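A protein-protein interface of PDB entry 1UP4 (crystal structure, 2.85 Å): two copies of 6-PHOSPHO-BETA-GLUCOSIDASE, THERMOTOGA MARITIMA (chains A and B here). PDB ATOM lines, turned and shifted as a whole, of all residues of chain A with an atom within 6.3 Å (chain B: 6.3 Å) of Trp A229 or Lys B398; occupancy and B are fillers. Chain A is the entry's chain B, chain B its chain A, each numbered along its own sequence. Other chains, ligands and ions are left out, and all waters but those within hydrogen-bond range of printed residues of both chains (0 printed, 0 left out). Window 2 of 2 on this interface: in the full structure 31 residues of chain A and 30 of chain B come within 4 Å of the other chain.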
ATOM      1  N   PRO A 227      12.288  10.168 -15.122  1.00  0.00           N
ATOM      2  CA  PRO A 227      13.667  10.608 -14.902  1.00  0.00           C
ATOM      3  C   PRO A 227      14.628   9.416 -14.950  1.00  0.00           C
ATOM      4  O   PRO A 227      14.187   8.272 -14.878  1.00  0.00           O
ATOM      5  CB  PRO A 227      13.636  11.192 -13.479  1.00  0.00           C
ATOM      6  CG  PRO A 227      12.252  11.053 -12.998  1.00  0.00           C
ATOM      7  CD  PRO A 227      11.540  10.072 -13.865  1.00  0.00           C
ATOM      8  N   THR A 228      15.924   9.689 -15.065  1.00  0.00           N
ATOM      9  CA  THR A 228      16.933   8.640 -15.057  1.00  0.00           C
ATOM     10  C   THR A 228      16.828   7.687 -13.865  1.00  0.00           C
ATOM     11  O   THR A 228      16.868   6.472 -14.055  1.00  0.00           O
ATOM     12  CB  THR A 228      18.309   9.257 -15.029  1.00  0.00           C
ATOM     13  OG1 THR A 228      18.579   9.844 -16.306  1.00  0.00           O
ATOM     14  CG2 THR A 228      19.368   8.157 -14.866  1.00  0.00           C
ATOM     15  N   TRP A 229      16.733   8.238 -12.645  1.00  0.00           N
ATOM     16  CA  TRP A 229      16.692   7.428 -11.420  1.00  0.00           C
ATOM     17  C   TRP A 229      15.548   6.414 -11.438  1.00  0.00           C
ATOM     18  O   TRP A 229      15.671   5.335 -10.867  1.00  0.00           O
ATOM     19  CB  TRP A 229      16.653   8.271 -10.126  1.00  0.00           C
ATOM     20  CG  TRP A 229      15.417   9.076  -9.940  1.00  0.00           C
ATOM     21  CD1 TRP A 229      15.245  10.398 -10.252  1.00  0.00           C
ATOM     22  CD2 TRP A 229      14.155   8.629  -9.416  1.00  0.00           C
ATOM     23  NE1 TRP A 229      13.961  10.799  -9.966  1.00  0.00           N
ATOM     24  CE2 TRP A 229      13.266   9.733  -9.455  1.00  0.00           C
ATOM     25  CE3 TRP A 229      13.675   7.405  -8.924  1.00  0.00           C
ATOM     26  CZ2 TRP A 229      11.934   9.643  -9.022  1.00  0.00           C
ATOM     27  CZ3 TRP A 229      12.347   7.318  -8.496  1.00  0.00           C
ATOM     28  CH2 TRP A 229      11.492   8.429  -8.552  1.00  0.00           C
ATOM     29  N   PHE A 230      14.442   6.758 -12.096  1.00  0.00           N
ATOM     30  CA  PHE A 230      13.313   5.867 -12.156  1.00  0.00           C
ATOM     31  C   PHE A 230      13.689   4.543 -12.823  1.00  0.00           C
ATOM     32  O   PHE A 230      13.299   3.467 -12.353  1.00  0.00           O
ATOM     33  CB  PHE A 230      12.134   6.529 -12.867  1.00  0.00           C
ATOM     34  CG  PHE A 230      10.944   5.645 -12.987  1.00  0.00           C
ATOM     35  CD1 PHE A 230      10.041   5.544 -11.937  1.00  0.00           C
ATOM     36  CD2 PHE A 230      10.753   4.875 -14.127  1.00  0.00           C
ATOM     37  CE1 PHE A 230       8.952   4.724 -12.019  1.00  0.00           C
ATOM     38  CE2 PHE A 230       9.657   4.036 -14.232  1.00  0.00           C
ATOM     39  CZ  PHE A 230       8.752   3.960 -13.178  1.00  0.00           C
ATOM     40  N   TYR A 231      14.445   4.621 -13.911  1.00  0.00           N
ATOM     41  CA  TYR A 231      14.831   3.434 -14.629  1.00  0.00           C
ATOM     42  C   TYR A 231      15.861   2.667 -13.819  1.00  0.00           C
ATOM     43  O   TYR A 231      15.838   1.449 -13.801  1.00  0.00           O
ATOM     44  CB  TYR A 231      15.305   3.792 -16.040  1.00  0.00           C
ATOM     45  CG  TYR A 231      14.193   4.287 -16.946  1.00  0.00           C
ATOM     46  CD1 TYR A 231      13.028   3.519 -17.154  1.00  0.00           C
ATOM     47  CD2 TYR A 231      14.295   5.525 -17.586  1.00  0.00           C
ATOM     48  CE1 TYR A 231      11.987   3.983 -17.997  1.00  0.00           C
ATOM     49  CE2 TYR A 231      13.289   6.000 -18.420  1.00  0.00           C
ATOM     50  CZ  TYR A 231      12.142   5.233 -18.623  1.00  0.00           C
ATOM     51  OH  TYR A 231      11.153   5.716 -19.451  1.00  0.00           O
ATOM     52  N   ASP A 232      16.735   3.386 -13.118  1.00  0.00           N
ATOM     53  CA  ASP A 232      17.731   2.755 -12.222  1.00  0.00           C
ATOM     54  C   ASP A 232      17.080   1.939 -11.106  1.00  0.00           C
ATOM     55  O   ASP A 232      17.607   0.909 -10.688  1.00  0.00           O
ATOM     56  CB  ASP A 232      18.592   3.792 -11.516  1.00  0.00           C
ATOM     57  CG  ASP A 232      19.606   4.401 -12.408  1.00  0.00           C
ATOM     58  OD1 ASP A 232      19.649   4.019 -13.600  1.00  0.00           O
ATOM     59  OD2 ASP A 232      20.390   5.286 -12.004  1.00  0.00           O
ATOM     60  N   SER A 233      15.943   2.423 -10.621  1.00  0.00           N
ATOM     61  CA  SER A 233      15.305   1.868  -9.449  1.00  0.00           C
ATOM     62  C   SER A 233      14.276   0.816  -9.805  1.00  0.00           C
ATOM     63  O   SER A 233      14.313  -0.293  -9.272  1.00  0.00           O
ATOM     64  CB  SER A 233      14.682   2.993  -8.637  1.00  0.00           C
ATOM     65  OG  SER A 233      15.644   4.040  -8.512  1.00  0.00           O
ATOM     66  N   VAL A 234      13.355   1.147 -10.702  1.00  0.00           N
ATOM     67  CA  VAL A 234      12.321   0.193 -11.072  1.00  0.00           C
ATOM     68  C   VAL A 234      12.888  -0.947 -11.963  1.00  0.00           C
ATOM     69  O   VAL A 234      12.454  -2.093 -11.853  1.00  0.00           O
ATOM     70  CB  VAL A 234      11.049   0.915 -11.646  1.00  0.00           C
ATOM     71  CG1 VAL A 234       9.975  -0.061 -12.009  1.00  0.00           C
ATOM     72  CG2 VAL A 234      10.471   1.892 -10.639  1.00  0.00           C
ATOM     73  N   LYS B 379      17.567   2.441  -3.843  1.00  0.00           N
ATOM     74  CA  LYS B 379      16.899   2.248  -5.130  1.00  0.00           C
ATOM     75  C   LYS B 379      15.662   1.388  -4.965  1.00  0.00           C
ATOM     76  O   LYS B 379      14.581   1.755  -5.427  1.00  0.00           O
ATOM     77  CB  LYS B 379      17.824   1.594  -6.171  1.00  0.00           C
ATOM     78  CG  LYS B 379      18.848   2.528  -6.854  1.00  0.00           C
ATOM     79  CD  LYS B 379      19.448   1.889  -8.128  1.00  0.00           C
ATOM     80  CE  LYS B 379      20.765   1.134  -7.881  1.00  0.00           C
ATOM     81  NZ  LYS B 379      21.954   2.014  -8.206  1.00  0.00           N
ATOM     82  N   LEU B 382      12.731   3.242  -3.065  1.00  0.00           N
ATOM     83  CA  LEU B 382      12.011   4.110  -3.990  1.00  0.00           C
ATOM     84  C   LEU B 382      10.973   3.303  -4.775  1.00  0.00           C
ATOM     85  O   LEU B 382       9.827   3.729  -4.937  1.00  0.00           O
ATOM     86  CB  LEU B 382      13.002   4.735  -4.946  1.00  0.00           C
ATOM     87  CG  LEU B 382      13.424   6.199  -4.916  1.00  0.00           C
ATOM     88  CD1 LEU B 382      12.825   7.005  -3.767  1.00  0.00           C
ATOM     89  CD2 LEU B 382      14.960   6.279  -4.977  1.00  0.00           C
ATOM     90  N   LYS B 383      11.374   2.128  -5.247  1.00  0.00           N
ATOM     91  CA  LYS B 383      10.467   1.268  -5.974  1.00  0.00           C
ATOM     92  C   LYS B 383       9.297   0.879  -5.060  1.00  0.00           C
ATOM     93  O   LYS B 383       8.118   0.914  -5.474  1.00  0.00           O
ATOM     94  CB  LYS B 383      11.195   0.035  -6.470  1.00  0.00           C
ATOM     95  CG  LYS B 383      10.327  -0.953  -7.172  1.00  0.00           C
ATOM     96  CD  LYS B 383      11.175  -2.071  -7.690  1.00  0.00           C
ATOM     97  CE  LYS B 383      10.511  -2.801  -8.835  1.00  0.00           C
ATOM     98  NZ  LYS B 383      11.329  -3.942  -9.255  1.00  0.00           N
ATOM     99  N   LEU B 386       6.969   3.942  -4.495  1.00  0.00           N
ATOM    100  CA  LEU B 386       6.118   4.189  -5.659  1.00  0.00           C
ATOM    101  C   LEU B 386       4.998   3.179  -5.833  1.00  0.00           C
ATOM    102  O   LEU B 386       3.991   3.469  -6.462  1.00  0.00           O
ATOM    103  CB  LEU B 386       6.925   4.262  -6.932  1.00  0.00           C
ATOM    104  CG  LEU B 386       7.800   5.488  -7.125  1.00  0.00           C
ATOM    105  CD1 LEU B 386       8.791   5.147  -8.190  1.00  0.00           C
ATOM    106  CD2 LEU B 386       6.978   6.683  -7.528  1.00  0.00           C
ATOM    107  N   PRO B 392       3.942   8.336  -3.042  1.00  0.00           N
ATOM    108  CA  PRO B 392       4.246   9.532  -3.812  1.00  0.00           C
ATOM    109  C   PRO B 392       4.172   9.324  -5.338  1.00  0.00           C
ATOM    110  O   PRO B 392       4.304   8.213  -5.816  1.00  0.00           O
ATOM    111  CB  PRO B 392       5.667   9.855  -3.369  1.00  0.00           C
ATOM    112  CG  PRO B 392       6.259   8.533  -3.030  1.00  0.00           C
ATOM    113  CD  PRO B 392       5.144   7.737  -2.440  1.00  0.00           C
ATOM    114  N   ASP B 393       3.916  10.410  -6.074  1.00  0.00           N
ATOM    115  CA  ASP B 393       4.169  10.481  -7.507  1.00  0.00           C
ATOM    116  C   ASP B 393       5.691  10.505  -7.686  1.00  0.00           C
ATOM    117  O   ASP B 393       6.462  10.859  -6.769  1.00  0.00           O
ATOM    118  CB  ASP B 393       3.587  11.771  -8.136  1.00  0.00           C
ATOM    119  CG  ASP B 393       2.050  11.710  -8.414  1.00  0.00           C
ATOM    120  OD1 ASP B 393       1.370  10.705  -8.093  1.00  0.00           O
ATOM    121  OD2 ASP B 393       1.427  12.660  -8.944  1.00  0.00           O
ATOM    122  N   VAL B 394       6.112  10.145  -8.894  1.00  0.00           N
ATOM    123  CA  VAL B 394       7.505  10.181  -9.288  1.00  0.00           C
ATOM    124  C   VAL B 394       8.201  11.505  -8.917  1.00  0.00           C
ATOM    125  O   VAL B 394       9.335  11.489  -8.441  1.00  0.00           O
ATOM    126  CB  VAL B 394       7.629   9.849 -10.775  1.00  0.00           C
ATOM    127  CG1 VAL B 394       8.999  10.114 -11.255  1.00  0.00           C
ATOM    128  CG2 VAL B 394       7.319   8.381 -11.002  1.00  0.00           C
ATOM    129  N   GLU B 395       7.520  12.636  -9.105  1.00  0.00           N
ATOM    130  CA  GLU B 395       8.100  13.949  -8.815  1.00  0.00           C
ATOM    131  C   GLU B 395       8.419  14.224  -7.329  1.00  0.00           C
ATOM    132  O   GLU B 395       9.231  15.098  -7.028  1.00  0.00           O
ATOM    133  CB  GLU B 395       7.244  15.063  -9.414  1.00  0.00           C
ATOM    134  CG  GLU B 395       5.845  15.222  -8.828  1.00  0.00           C
ATOM    135  CD  GLU B 395       5.022  16.307  -9.523  1.00  0.00           C
ATOM    136  OE1 GLU B 395       5.398  17.497  -9.465  1.00  0.00           O
ATOM    137  OE2 GLU B 395       3.985  15.980 -10.140  1.00  0.00           O
ATOM    138  N   ASP B 396       7.814  13.461  -6.425  1.00  0.00           N
ATOM    139  CA  ASP B 396       7.998  13.644  -5.002  1.00  0.00           C
ATOM    140  C   ASP B 396       8.774  12.533  -4.300  1.00  0.00           C
ATOM    141  O   ASP B 396       9.269  12.723  -3.188  1.00  0.00           O
ATOM    142  CB  ASP B 396       6.648  13.809  -4.347  1.00  0.00           C
ATOM    143  CG  ASP B 396       6.044  15.162  -4.623  1.00  0.00           C
ATOM    144  OD1 ASP B 396       6.829  16.122  -4.775  1.00  0.00           O
ATOM    145  OD2 ASP B 396       4.814  15.374  -4.725  1.00  0.00           O
ATOM    146  N   ALA B 397       8.902  11.385  -4.961  1.00  0.00           N
ATOM    147  CA  ALA B 397       9.410  10.175  -4.342  1.00  0.00           C
ATOM    148  C   ALA B 397      10.802  10.319  -3.745  1.00  0.00           C
ATOM    149  O   ALA B 397      11.002   9.960  -2.616  1.00  0.00           O
ATOM    150  CB  ALA B 397       9.336   9.038  -5.319  1.00  0.00           C
ATOM    151  N   LYS B 398      11.758  10.844  -4.504  1.00  0.00           N
ATOM    152  CA  LYS B 398      13.155  10.981  -4.078  1.00  0.00           C
ATOM    153  C   LYS B 398      13.313  11.886  -2.845  1.00  0.00           C
ATOM    154  O   LYS B 398      13.963  11.521  -1.871  1.00  0.00           O
ATOM    155  CB  LYS B 398      13.973  11.548  -5.227  1.00  0.00           C
ATOM    156  CG  LYS B 398      14.998  10.611  -5.804  1.00  0.00           C
ATOM    157  CD  LYS B 398      16.085  11.396  -6.553  1.00  0.00           C
ATOM    158  CE  LYS B 398      17.373  10.576  -6.676  1.00  0.00           C
ATOM    159  NZ  LYS B 398      18.268  10.690  -5.478  1.00  0.00           N
ATOM    160  N   ASP B 399      12.704  13.065  -2.895  1.00  0.00           N
ATOM    161  CA  ASP B 399      12.664  13.959  -1.762  1.00  0.00           C
ATOM    162  C   ASP B 399      11.988  13.351  -0.522  1.00  0.00           C
ATOM    163  O   ASP B 399      12.474  13.513   0.605  1.00  0.00           O
ATOM    164  CB  ASP B 399      11.963  15.231  -2.192  1.00  0.00           C
ATOM    165  CG  ASP B 399      12.797  16.049  -3.175  1.00  0.00           C
ATOM    166  OD1 ASP B 399      14.025  15.788  -3.288  1.00  0.00           O
ATOM    167  OD2 ASP B 399      12.310  16.976  -3.875  1.00  0.00           O
ATOM    168  N   LEU B 400      10.874  12.660  -0.726  1.00  0.00           N
ATOM    169  CA  LEU B 400      10.180  12.032   0.377  1.00  0.00           C
ATOM    170  C   LEU B 400      11.055  10.978   1.059  1.00  0.00           C
ATOM    171  O   LEU B 400      11.191  10.984   2.296  1.00  0.00           O
ATOM    172  CB  LEU B 400       8.835  11.444  -0.072  1.00  0.00           C
ATOM    173  CG  LEU B 400       7.996  10.634   0.930  1.00  0.00           C
ATOM    174  CD1 LEU B 400       7.506  11.433   2.139  1.00  0.00           C
ATOM    175  CD2 LEU B 400       6.825   9.994   0.224  1.00  0.00           C
ATOM    176  N   LEU B 401      11.661  10.096   0.258  1.00  0.00           N
ATOM    177  CA  LEU B 401      12.501   9.034   0.794  1.00  0.00           C
ATOM    178  C   LEU B 401      13.685   9.598   1.568  1.00  0.00           C
ATOM    179  O   LEU B 401      13.995   9.104   2.649  1.00  0.00           O
ATOM    180  CB  LEU B 401      12.947   8.056  -0.282  1.00  0.00           C
ATOM    181  CG  LEU B 401      13.817   6.888   0.215  1.00  0.00           C
ATOM    182  CD1 LEU B 401      13.187   6.117   1.380  1.00  0.00           C
ATOM    183  CD2 LEU B 401      14.174   5.933  -0.901  1.00  0.00           C
ATOM    184  N   GLU B 402      14.303  10.650   1.040  1.00  0.00           N
ATOM    185  CA  GLU B 402      15.389  11.321   1.728  1.00  0.00           C
ATOM    186  C   GLU B 402      14.995  11.893   3.085  1.00  0.00           C
ATOM    187  O   GLU B 402      15.751  11.781   4.054  1.00  0.00           O
ATOM    188  CB  GLU B 402      16.000  12.364   0.817  1.00  0.00           C
ATOM    189  CG  GLU B 402      16.724  11.691  -0.354  1.00  0.00           C
ATOM    190  CD  GLU B 402      17.221  12.662  -1.431  1.00  0.00           C
ATOM    191  OE1 GLU B 402      16.847  13.876  -1.392  1.00  0.00           O
ATOM    192  OE2 GLU B 402      17.994  12.191  -2.324  1.00  0.00           O
ATOM    193  N   GLU B 403      13.799  12.476   3.167  1.00  0.00           N
ATOM    194  CA  GLU B 403      13.280  12.971   4.444  1.00  0.00           C
ATOM    195  C   GLU B 403      13.050  11.845   5.442  1.00  0.00           C
ATOM    196  O   GLU B 403      13.362  11.995   6.622  1.00  0.00           O
ATOM    197  CB  GLU B 403      11.983  13.758   4.287  1.00  0.00           C
ATOM    198  CG  GLU B 403      12.170  15.235   4.561  1.00  0.00           C
ATOM    199  CD  GLU B 403      10.894  16.020   4.844  1.00  0.00           C
ATOM    200  OE1 GLU B 403       9.847  15.769   4.211  1.00  0.00           O
ATOM    201  OE2 GLU B 403      10.976  16.948   5.693  1.00  0.00           O
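The side-chain amino group (NZ) of Lys B383 lies within hydrogen-bond range of the backbone carbonyl oxygen (O) of Val A234 (3.4 Å).
The side-chain carboxylate (OE2) of Glu B402 is in salt-bridge range of the side-chain amino group (NZ) of Lys B398 (3.5 Å). O of Trp A229 sits at hydrogen-bond distance from OG of Ser A233 (2.7 Å).
Among the printed residues, pairs that only touch across the chains: Trp A229 with Val B394, Asp A232 with Lys B379, Ser A233 with Lys B379, Pro A227 with Val B394, Phe A230 with Leu B386, Trp A229 with Leu B382, Trp A229 with Lys B398, Trp A229 with Ala B397 and Ser A233 with Lys B383.
Printed residues of chain B within 4 Å of Pro A227: Val B394 (3.6 Å). Trp A229 touches just these residues of chain B: Leu B382, Val B394, Ala B397 and Lys B398. Printed residues of chain A within 4 Å of Lys B379: Asp A232 (3.3 Å) and Ser A233 (3.4 Å). Of the printed residues of chain A, Ala B397 touches Trp A229. Lys B398 touches just one residue of chain A: Trp A229. The nearest residue of chain B that does not touch Trp A229 is Leu B386 (4.2 Å). The nearest printed residue of chain B that does not touch Pro A227 is Glu B395 (6.3 Å).
Printed residues of chain A that touch a printed residue of chain B: Pro A227, Trp A229, Phe A230, Asp A232, Ser A233 and Val A234. Hydrophobic or aromatic side chains of chain A that line the printed part of chain B: Pro A227, Trp A229 and Phe A230. Among the printed residues, 10 pairs touch across the chains.
No position is printed for both chains. Of the 10 pairs that touch across the chains among the printed residues, none has its exchanged pair printed and touching as well.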
